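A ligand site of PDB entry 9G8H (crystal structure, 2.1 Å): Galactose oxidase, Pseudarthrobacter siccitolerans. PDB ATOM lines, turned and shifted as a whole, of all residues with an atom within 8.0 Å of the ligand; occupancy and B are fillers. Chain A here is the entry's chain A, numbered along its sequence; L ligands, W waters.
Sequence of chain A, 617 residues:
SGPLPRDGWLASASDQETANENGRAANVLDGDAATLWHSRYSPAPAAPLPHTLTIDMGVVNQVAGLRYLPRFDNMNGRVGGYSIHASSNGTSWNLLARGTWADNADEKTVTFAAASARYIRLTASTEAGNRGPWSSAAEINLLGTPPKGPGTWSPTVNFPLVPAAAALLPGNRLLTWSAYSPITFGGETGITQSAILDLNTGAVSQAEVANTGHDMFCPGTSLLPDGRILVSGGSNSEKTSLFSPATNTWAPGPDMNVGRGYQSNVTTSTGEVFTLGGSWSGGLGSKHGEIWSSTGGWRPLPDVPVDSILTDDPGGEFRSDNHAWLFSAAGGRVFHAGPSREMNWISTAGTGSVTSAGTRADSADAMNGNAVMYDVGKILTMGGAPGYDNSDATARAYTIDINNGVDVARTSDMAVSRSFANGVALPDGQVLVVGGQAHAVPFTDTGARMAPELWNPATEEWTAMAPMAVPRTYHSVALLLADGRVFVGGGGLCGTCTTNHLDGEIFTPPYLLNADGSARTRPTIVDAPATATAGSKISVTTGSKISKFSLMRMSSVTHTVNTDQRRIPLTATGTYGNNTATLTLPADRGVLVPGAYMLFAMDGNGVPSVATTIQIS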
ATOM      1  N   GLU A  17      34.498 -10.277   1.284  1.00  0.00           N
ATOM      2  CA  GLU A  17      33.745 -10.162   0.054  1.00  0.00           C
ATOM      3  C   GLU A  17      34.030  -8.816  -0.612  1.00  0.00           C
ATOM      4  O   GLU A  17      34.172  -7.781   0.057  1.00  0.00           O
ATOM      5  CB  GLU A  17      32.268 -10.355   0.366  1.00  0.00           C
ATOM      6  CG  GLU A  17      31.379 -10.311  -0.856  1.00  0.00           C
ATOM      7  CD  GLU A  17      31.581 -11.510  -1.772  1.00  0.00           C
ATOM      8  OE1 GLU A  17      32.130 -12.540  -1.305  1.00  0.00           O
ATOM      9  OE2 GLU A  17      31.228 -11.388  -2.952  1.00  0.00           O
ATOM     10  N   ASN A  20      30.343  -9.518  -4.704  1.00  0.00           N
ATOM     11  CA  ASN A  20      28.886  -9.424  -4.712  1.00  0.00           C
ATOM     12  C   ASN A  20      28.372  -8.219  -3.913  1.00  0.00           C
ATOM     13  O   ASN A  20      27.218  -7.851  -4.061  1.00  0.00           O
ATOM     14  CB  ASN A  20      28.229 -10.683  -4.150  1.00  0.00           C
ATOM     15  CG  ASN A  20      26.721 -10.584  -4.216  1.00  0.00           C
ATOM     16  OD1 ASN A  20      26.027 -10.900  -3.254  1.00  0.00           O
ATOM     17  ND2 ASN A  20      26.206 -10.128  -5.350  1.00  0.00           N
ATOM     18  N   GLU A  21      29.233  -7.656  -3.050  1.00  0.00           N
ATOM     19  CA  GLU A  21      29.009  -6.375  -2.375  1.00  0.00           C
ATOM     20  C   GLU A  21      30.365  -5.895  -1.893  1.00  0.00           C
ATOM     21  O   GLU A  21      31.374  -6.595  -2.089  1.00  0.00           O
ATOM     22  CB  GLU A  21      28.033  -6.511  -1.200  1.00  0.00           C
ATOM     23  CG  GLU A  21      28.573  -7.418  -0.116  1.00  0.00           C
ATOM     24  CD  GLU A  21      27.683  -7.737   1.080  1.00  0.00           C
ATOM     25  OE1 GLU A  21      27.296  -6.806   1.808  1.00  0.00           O
ATOM     26  OE2 GLU A  21      27.404  -8.929   1.296  1.00  0.00           O
ATOM     27  N   LEU A  36      29.787  -2.627   5.745  1.00  0.00           N
ATOM     28  CA  LEU A  36      30.120  -3.843   6.483  1.00  0.00           C
ATOM     29  C   LEU A  36      31.452  -4.426   6.028  1.00  0.00           C
ATOM     30  O   LEU A  36      31.828  -4.295   4.855  1.00  0.00           O
ATOM     31  CB  LEU A  36      29.078  -4.943   6.211  1.00  0.00           C
ATOM     32  CG  LEU A  36      27.601  -4.588   6.233  1.00  0.00           C
ATOM     33  CD1 LEU A  36      26.771  -5.832   5.939  1.00  0.00           C
ATOM     34  CD2 LEU A  36      27.204  -3.989   7.583  1.00  0.00           C
ATOM     35  N   TRP A  37      32.109  -5.115   6.972  1.00  0.00           N
ATOM     36  CA  TRP A  37      32.986  -6.223   6.647  1.00  0.00           C
ATOM     37  C   TRP A  37      32.152  -7.492   6.573  1.00  0.00           C
ATOM     38  O   TRP A  37      31.412  -7.811   7.512  1.00  0.00           O
ATOM     39  CB  TRP A  37      34.100  -6.395   7.698  1.00  0.00           C
ATOM     40  CG  TRP A  37      34.789  -7.723   7.571  1.00  0.00           C
ATOM     41  CD1 TRP A  37      35.532  -8.167   6.507  1.00  0.00           C
ATOM     42  CD2 TRP A  37      34.804  -8.803   8.538  1.00  0.00           C
ATOM     43  NE1 TRP A  37      36.017  -9.428   6.751  1.00  0.00           N
ATOM     44  CE2 TRP A  37      35.591  -9.853   7.990  1.00  0.00           C
ATOM     45  CE3 TRP A  37      34.241  -8.986   9.813  1.00  0.00           C
ATOM     46  CZ2 TRP A  37      35.824 -11.050   8.661  1.00  0.00           C
ATOM     47  CZ3 TRP A  37      34.483 -10.165  10.493  1.00  0.00           C
ATOM     48  CH2 TRP A  37      35.266 -11.176   9.918  1.00  0.00           C
ATOM     49  N   HIS A  38      32.243  -8.185   5.427  1.00  0.00           N
ATOM     50  CA  HIS A  38      31.639  -9.507   5.294  1.00  0.00           C
ATOM     51  C   HIS A  38      32.716 -10.469   4.818  1.00  0.00           C
ATOM     52  O   HIS A  38      33.544 -10.112   3.964  1.00  0.00           O
ATOM     53  CB  HIS A  38      30.413  -9.478   4.370  1.00  0.00           C
ATOM     54  CG  HIS A  38      29.469 -10.649   4.494  1.00  0.00           C
ATOM     55  ND1 HIS A  38      29.835 -11.967   4.324  1.00  0.00           N
ATOM     56  CD2 HIS A  38      28.165 -10.678   4.793  1.00  0.00           C
ATOM     57  CE1 HIS A  38      28.785 -12.749   4.511  1.00  0.00           C
ATOM     58  NE2 HIS A  38      27.761 -11.985   4.784  1.00  0.00           N
ATOM     59  N   SER A  39      32.732 -11.670   5.404  1.00  0.00           N
ATOM     60  CA  SER A  39      33.584 -12.744   4.950  1.00  0.00           C
ATOM     61  C   SER A  39      33.299 -13.067   3.480  1.00  0.00           C
ATOM     62  O   SER A  39      32.191 -12.822   2.996  1.00  0.00           O
ATOM     63  CB  SER A  39      33.431 -13.972   5.824  1.00  0.00           C
ATOM     64  OG  SER A  39      32.063 -14.322   5.969  1.00  0.00           O
ATOM     65  N   ARG A  40      34.303 -13.620   2.781  1.00  0.00           N
ATOM     66  CA  ARG A  40      34.202 -13.962   1.364  1.00  0.00           C
ATOM     67  C   ARG A  40      33.250 -15.143   1.162  1.00  0.00           C
ATOM     68  O   ARG A  40      33.405 -16.182   1.787  1.00  0.00           O
ATOM     69  CB  ARG A  40      35.562 -14.343   0.765  1.00  0.00           C
ATOM     70  CG  ARG A  40      35.564 -14.363  -0.753  1.00  0.00           C
ATOM     71  CD  ARG A  40      36.867 -14.904  -1.326  1.00  0.00           C
ATOM     72  NE  ARG A  40      37.027 -16.300  -0.920  1.00  0.00           N
ATOM     73  CZ  ARG A  40      36.344 -17.346  -1.402  1.00  0.00           C
ATOM     74  NH1 ARG A  40      35.415 -17.190  -2.332  1.00  0.00           N
ATOM     75  NH2 ARG A  40      36.594 -18.543  -0.939  1.00  0.00           N
ATOM     76  N   TYR A  41      32.275 -14.944   0.276  1.00  0.00           N
ATOM     77  CA  TYR A  41      31.285 -15.975   0.012  1.00  0.00           C
ATOM     78  C   TYR A  41      31.218 -16.299  -1.476  1.00  0.00           C
ATOM     79  O   TYR A  41      30.713 -17.350  -1.838  1.00  0.00           O
ATOM     80  CB  TYR A  41      29.947 -15.758   0.729  1.00  0.00           C
ATOM     81  CG  TYR A  41      29.235 -14.463   0.337  1.00  0.00           C
ATOM     82  CD1 TYR A  41      28.488 -14.363  -0.837  1.00  0.00           C
ATOM     83  CD2 TYR A  41      29.351 -13.328   1.143  1.00  0.00           C
ATOM     84  CE1 TYR A  41      27.851 -13.175  -1.184  1.00  0.00           C
ATOM     85  CE2 TYR A  41      28.741 -12.139   0.787  1.00  0.00           C
ATOM     86  CZ  TYR A  41      27.985 -12.062  -0.374  1.00  0.00           C
ATOM     87  OH  TYR A  41      27.381 -10.867  -0.669  1.00  0.00           O
ATOM     88  N   SER A  42      31.775 -15.419  -2.326  1.00  0.00           N
ATOM     89  CA  SER A  42      31.783 -15.677  -3.761  1.00  0.00           C
ATOM     90  C   SER A  42      33.204 -15.571  -4.293  1.00  0.00           C
ATOM     91  O   SER A  42      34.003 -14.799  -3.762  1.00  0.00           O
ATOM     92  CB  SER A  42      30.836 -14.756  -4.483  1.00  0.00           C
ATOM     93  OG  SER A  42      31.321 -13.425  -4.498  1.00  0.00           O
ATOM     94  N   ALA A  46      32.234 -20.505  -0.741  1.00  0.00           N
ATOM     95  CA  ALA A  46      32.380 -19.478   0.281  1.00  0.00           C
ATOM     96  C   ALA A  46      33.522 -19.885   1.199  1.00  0.00           C
ATOM     97  O   ALA A  46      33.782 -21.085   1.347  1.00  0.00           O
ATOM     98  CB  ALA A  46      31.091 -19.325   1.042  1.00  0.00           C
ATOM     99  N   ARG A  71      25.474  -5.462  11.405  1.00  0.00           N
ATOM    100  CA  ARG A  71      24.654  -4.893  10.342  1.00  0.00           C
ATOM    101  C   ARG A  71      23.212  -4.701  10.843  1.00  0.00           C
ATOM    102  O   ARG A  71      22.816  -5.312  11.836  1.00  0.00           O
ATOM    103  CB  ARG A  71      24.689  -5.800   9.107  1.00  0.00           C
ATOM    104  CG  ARG A  71      24.114  -7.200   9.322  1.00  0.00           C
ATOM    105  CD  ARG A  71      24.414  -8.236   8.243  1.00  0.00           C
ATOM    106  NE  ARG A  71      24.069  -7.747   6.915  1.00  0.00           N
ATOM    107  CZ  ARG A  71      24.373  -8.354   5.768  1.00  0.00           C
ATOM    108  NH1 ARG A  71      24.915  -9.558   5.781  1.00  0.00           N
ATOM    109  NH2 ARG A  71      24.111  -7.745   4.612  1.00  0.00           N
ATOM    110  N   ASP A  73      20.676  -4.551   8.236  1.00  0.00           N
ATOM    111  CA  ASP A  73      19.857  -4.863   7.066  1.00  0.00           C
ATOM    112  C   ASP A  73      19.300  -6.293   7.112  1.00  0.00           C
ATOM    113  O   ASP A  73      18.216  -6.539   6.568  1.00  0.00           O
ATOM    114  CB  ASP A  73      20.636  -4.601   5.779  1.00  0.00           C
ATOM    115  CG  ASP A  73      21.967  -5.317   5.771  1.00  0.00           C
ATOM    116  OD1 ASP A  73      22.592  -5.401   6.854  1.00  0.00           O
ATOM    117  OD2 ASP A  73      22.387  -5.756   4.687  1.00  0.00           O
ATOM    118  N   ASN A  74      20.024  -7.233   7.733  1.00  0.00           N
ATOM    119  CA  ASN A  74      19.622  -8.637   7.861  1.00  0.00           C
ATOM    120  C   ASN A  74      20.497  -9.318   8.913  1.00  0.00           C
ATOM    121  O   ASN A  74      21.223  -8.637   9.647  1.00  0.00           O
ATOM    122  CB  ASN A  74      19.550  -9.380   6.521  1.00  0.00           C
ATOM    123  CG  ASN A  74      20.890  -9.539   5.818  1.00  0.00           C
ATOM    124  OD1 ASN A  74      21.798 -10.163   6.353  1.00  0.00           O
ATOM    125  ND2 ASN A  74      21.015  -8.993   4.620  1.00  0.00           N
ATOM    126  N   MET A  75      20.430 -10.645   8.984  1.00  0.00           N
ATOM    127  CA  MET A  75      20.999 -11.326  10.148  1.00  0.00           C
ATOM    128  C   MET A  75      22.304 -12.053   9.782  1.00  0.00           C
ATOM    129  O   MET A  75      23.013 -12.549  10.649  1.00  0.00           O
ATOM    130  CB  MET A  75      19.974 -12.287  10.760  1.00  0.00           C
ATOM    131  CG  MET A  75      18.684 -11.591  11.206  1.00  0.00           C
ATOM    132  SD  MET A  75      17.258 -12.641  11.600  1.00  0.00           S
ATOM    133  CE  MET A  75      17.514 -13.987  10.448  1.00  0.00           C
ATOM    134  N   ASN A  76      22.629 -12.074   8.479  1.00  0.00           N
ATOM    135  CA  ASN A  76      23.694 -12.908   7.947  1.00  0.00           C
ATOM    136  C   ASN A  76      25.041 -12.472   8.484  1.00  0.00           C
ATOM    137  O   ASN A  76      25.560 -11.422   8.111  1.00  0.00           O
ATOM    138  CB  ASN A  76      23.715 -12.905   6.421  1.00  0.00           C
ATOM    139  CG  ASN A  76      22.586 -13.699   5.804  1.00  0.00           C
ATOM    140  OD1 ASN A  76      21.812 -14.334   6.526  1.00  0.00           O
ATOM    141  ND2 ASN A  76      22.504 -13.702   4.476  1.00  0.00           N
ATOM    142  N   GLY A  77      25.614 -13.295   9.353  1.00  0.00           N
ATOM    143  CA  GLY A  77      27.016 -13.157   9.675  1.00  0.00           C
ATOM    144  C   GLY A  77      27.238 -12.527  11.038  1.00  0.00           C
ATOM    145  O   GLY A  77      28.384 -12.352  11.448  1.00  0.00           O
ATOM    146  N   GLU A 127      28.391 -18.330  13.429  1.00  0.00           N
ATOM    147  CA  GLU A 127      27.375 -17.386  12.986  1.00  0.00           C
ATOM    148  C   GLU A 127      26.191 -17.574  13.944  1.00  0.00           C
ATOM    149  O   GLU A 127      25.733 -18.698  14.112  1.00  0.00           O
ATOM    150  CB  GLU A 127      27.037 -17.722  11.533  1.00  0.00           C
ATOM    151  CG  GLU A 127      26.320 -16.627  10.749  1.00  0.00           C
ATOM    152  CD  GLU A 127      24.819 -16.500  10.898  1.00  0.00           C
ATOM    153  OE1 GLU A 127      24.195 -17.342  11.564  1.00  0.00           O
ATOM    154  OE2 GLU A 127      24.253 -15.512  10.356  1.00  0.00           O
ATOM    155  N   GLY A 132      24.887 -19.884   8.108  1.00  0.00           N
ATOM    156  CA  GLY A 132      25.855 -20.031   7.032  1.00  0.00           C
ATOM    157  C   GLY A 132      27.265 -19.811   7.559  1.00  0.00           C
ATOM    158  O   GLY A 132      27.431 -19.438   8.720  1.00  0.00           O
ATOM    159  N   PRO A 133      28.308 -20.027   6.709  1.00  0.00           N
ATOM    160  CA  PRO A 133      29.701 -19.879   7.153  1.00  0.00           C
ATOM    161  C   PRO A 133      30.193 -18.429   7.159  1.00  0.00           C
ATOM    162  O   PRO A 133      31.301 -18.149   6.664  1.00  0.00           O
ATOM    163  CB  PRO A 133      30.417 -20.695   6.056  1.00  0.00           C
ATOM    164  CG  PRO A 133      29.628 -20.338   4.810  1.00  0.00           C
ATOM    165  CD  PRO A 133      28.198 -20.421   5.296  1.00  0.00           C
ATOM    166  N   TRP A 134      29.380 -17.516   7.719  1.00  0.00           N
ATOM    167  CA  TRP A 134      29.572 -16.086   7.551  1.00  0.00           C
ATOM    168  C   TRP A 134      29.902 -15.396   8.868  1.00  0.00           C
ATOM    169  O   TRP A 134      29.396 -15.774   9.931  1.00  0.00           O
ATOM    170  CB  TRP A 134      28.309 -15.455   6.946  1.00  0.00           C
ATOM    171  CG  TRP A 134      27.808 -16.092   5.683  1.00  0.00           C
ATOM    172  CD1 TRP A 134      28.511 -16.414   4.550  1.00  0.00           C
ATOM    173  CD2 TRP A 134      26.441 -16.484   5.421  1.00  0.00           C
ATOM    174  NE1 TRP A 134      27.684 -16.970   3.614  1.00  0.00           N
ATOM    175  CE2 TRP A 134      26.415 -17.031   4.116  1.00  0.00           C
ATOM    176  CE3 TRP A 134      25.266 -16.433   6.168  1.00  0.00           C
ATOM    177  CZ2 TRP A 134      25.241 -17.526   3.548  1.00  0.00           C
ATOM    178  CZ3 TRP A 134      24.110 -16.921   5.610  1.00  0.00           C
ATOM    179  CH2 TRP A 134      24.111 -17.472   4.317  1.00  0.00           C
ATOM    180  N   SER A 135      30.749 -14.352   8.769  1.00  0.00           N
ATOM    181  CA  SER A 135      30.949 -13.287   9.759  1.00  0.00           C
ATOM    182  C   SER A 135      30.741 -11.938   9.057  1.00  0.00           C
ATOM    183  O   SER A 135      31.077 -11.794   7.878  1.00  0.00           O
ATOM    184  CB  SER A 135      32.323 -13.345  10.373  1.00  0.00           C
ATOM    185  OG  SER A 135      32.646 -14.641  10.814  1.00  0.00           O
ATOM    186  N   SER A 136      30.203 -10.968   9.811  1.00  0.00           N
ATOM    187  CA  SER A 136      30.032  -9.603   9.324  1.00  0.00           C
ATOM    188  C   SER A 136      30.051  -8.618  10.491  1.00  0.00           C
ATOM    189  O   SER A 136      29.708  -8.975  11.616  1.00  0.00           O
ATOM    190  CB  SER A 136      28.774  -9.443   8.462  1.00  0.00           C
ATOM    191  OG  SER A 136      27.588  -9.706   9.184  1.00  0.00           O
HETATM  192  C1  LIG L   1      22.994 -11.858   1.204  1.00  0.00           C
HETATM  193  C2  LIG L   1      23.435 -10.770   2.158  1.00  0.00           C
HETATM  194  C3  LIG L   1      24.967 -10.647   2.118  1.00  0.00           C
HETATM  195  C4  LIG L   1      25.603 -11.983   2.396  1.00  0.00           C
HETATM  196  C5  LIG L   1      25.100 -12.978   1.365  1.00  0.00           C
HETATM  197  C6  LIG L   1      25.624 -14.375   1.528  1.00  0.00           C
HETATM  198  O1  LIG L   1      21.657 -12.063   1.423  1.00  0.00           O
HETATM  199  O2  LIG L   1      22.733  -9.572   1.861  1.00  0.00           O
HETATM  200  O3  LIG L   1      25.440  -9.680   3.059  1.00  0.00           O
HETATM  201  O4  LIG L   1      25.232 -12.436   3.700  1.00  0.00           O
HETATM  202  O5  LIG L   1      23.665 -13.070   1.517  1.00  0.00           O
HETATM  203  O6  LIG L   1      24.834 -15.240   0.706  1.00  0.00           O
HETATM  204  O   HOH W   1      24.489  -7.186   1.332  1.00  0.00           O
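Water W1 lies within hydrogen-bond range of the side-chain carboxylate of Glu 21, an oxygen (O2) of the ligand and the guanidinium group of Arg 71.
An oxygen (O2) of the ligand lies within hydrogen-bond range of the side-chain amide nitrogen (ND2) of Asn 74 (3.3 Å).
The guanidinium group of Arg 71 sits at hydrogen-bond distance from an oxygen (O3) of the ligand, 2.8 Å away.
The side-chain carboxylate (OE2) of Glu 21 is in hydrogen-bond range of an oxygen (O3) of the ligand (2.7 Å).
An oxygen (O4) of the ligand is in hydrogen-bond range of the side-chain amide nitrogen of Asn 76 (3.1 Å).
NE2 of His 38 lies within hydrogen-bond range of O4 of the ligand, at 2.8 Å.
The guanidinium group (NH2) of Arg 71 lies within salt-bridge range of the side-chain carboxylate (OD2) of Asp 73 (2.6 Å).
N of Glu 17 lies within hydrogen-bond range of O of His 38 (2.8 Å).
N of Asn 76 sits at hydrogen-bond distance from OD1 of Asn 74 (3.0 Å).
The guanidinium group (NH1) of Arg 71 lies close to the side-chain amide oxygen (OD1) of Asn 74 (3.2 Å).
NH1 of Arg 71 is in hydrogen-bond range of O of Asn 76, at 3.1 Å.
The backbone carbonyl oxygen (O) of Asn 76 lies within hydrogen-bond range of the side-chain hydroxyl (OG) of Ser 136 (2.9 Å).
The side-chain carboxylate (OE2) of Glu 21 is in hydrogen-bond range of the side-chain hydroxyl (OH) of Tyr 41, at 2.8 Å.
The backbone NH (N) of Tyr 41 lies within hydrogen-bond range of the side-chain carboxylate (OE1) of Glu 17.
Tyr 41 touches the ligand (CZ to C5, 3.5 Å).
Trp 134 touches the ligand (CZ2 to O6, 3.7 Å).
Hydrophobic or aromatic side chains that line the ligand: His 38, Tyr 41 and Trp 134.
The nearest printed residue that does not touch the ligand is Asp 73 (4.8 Å).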
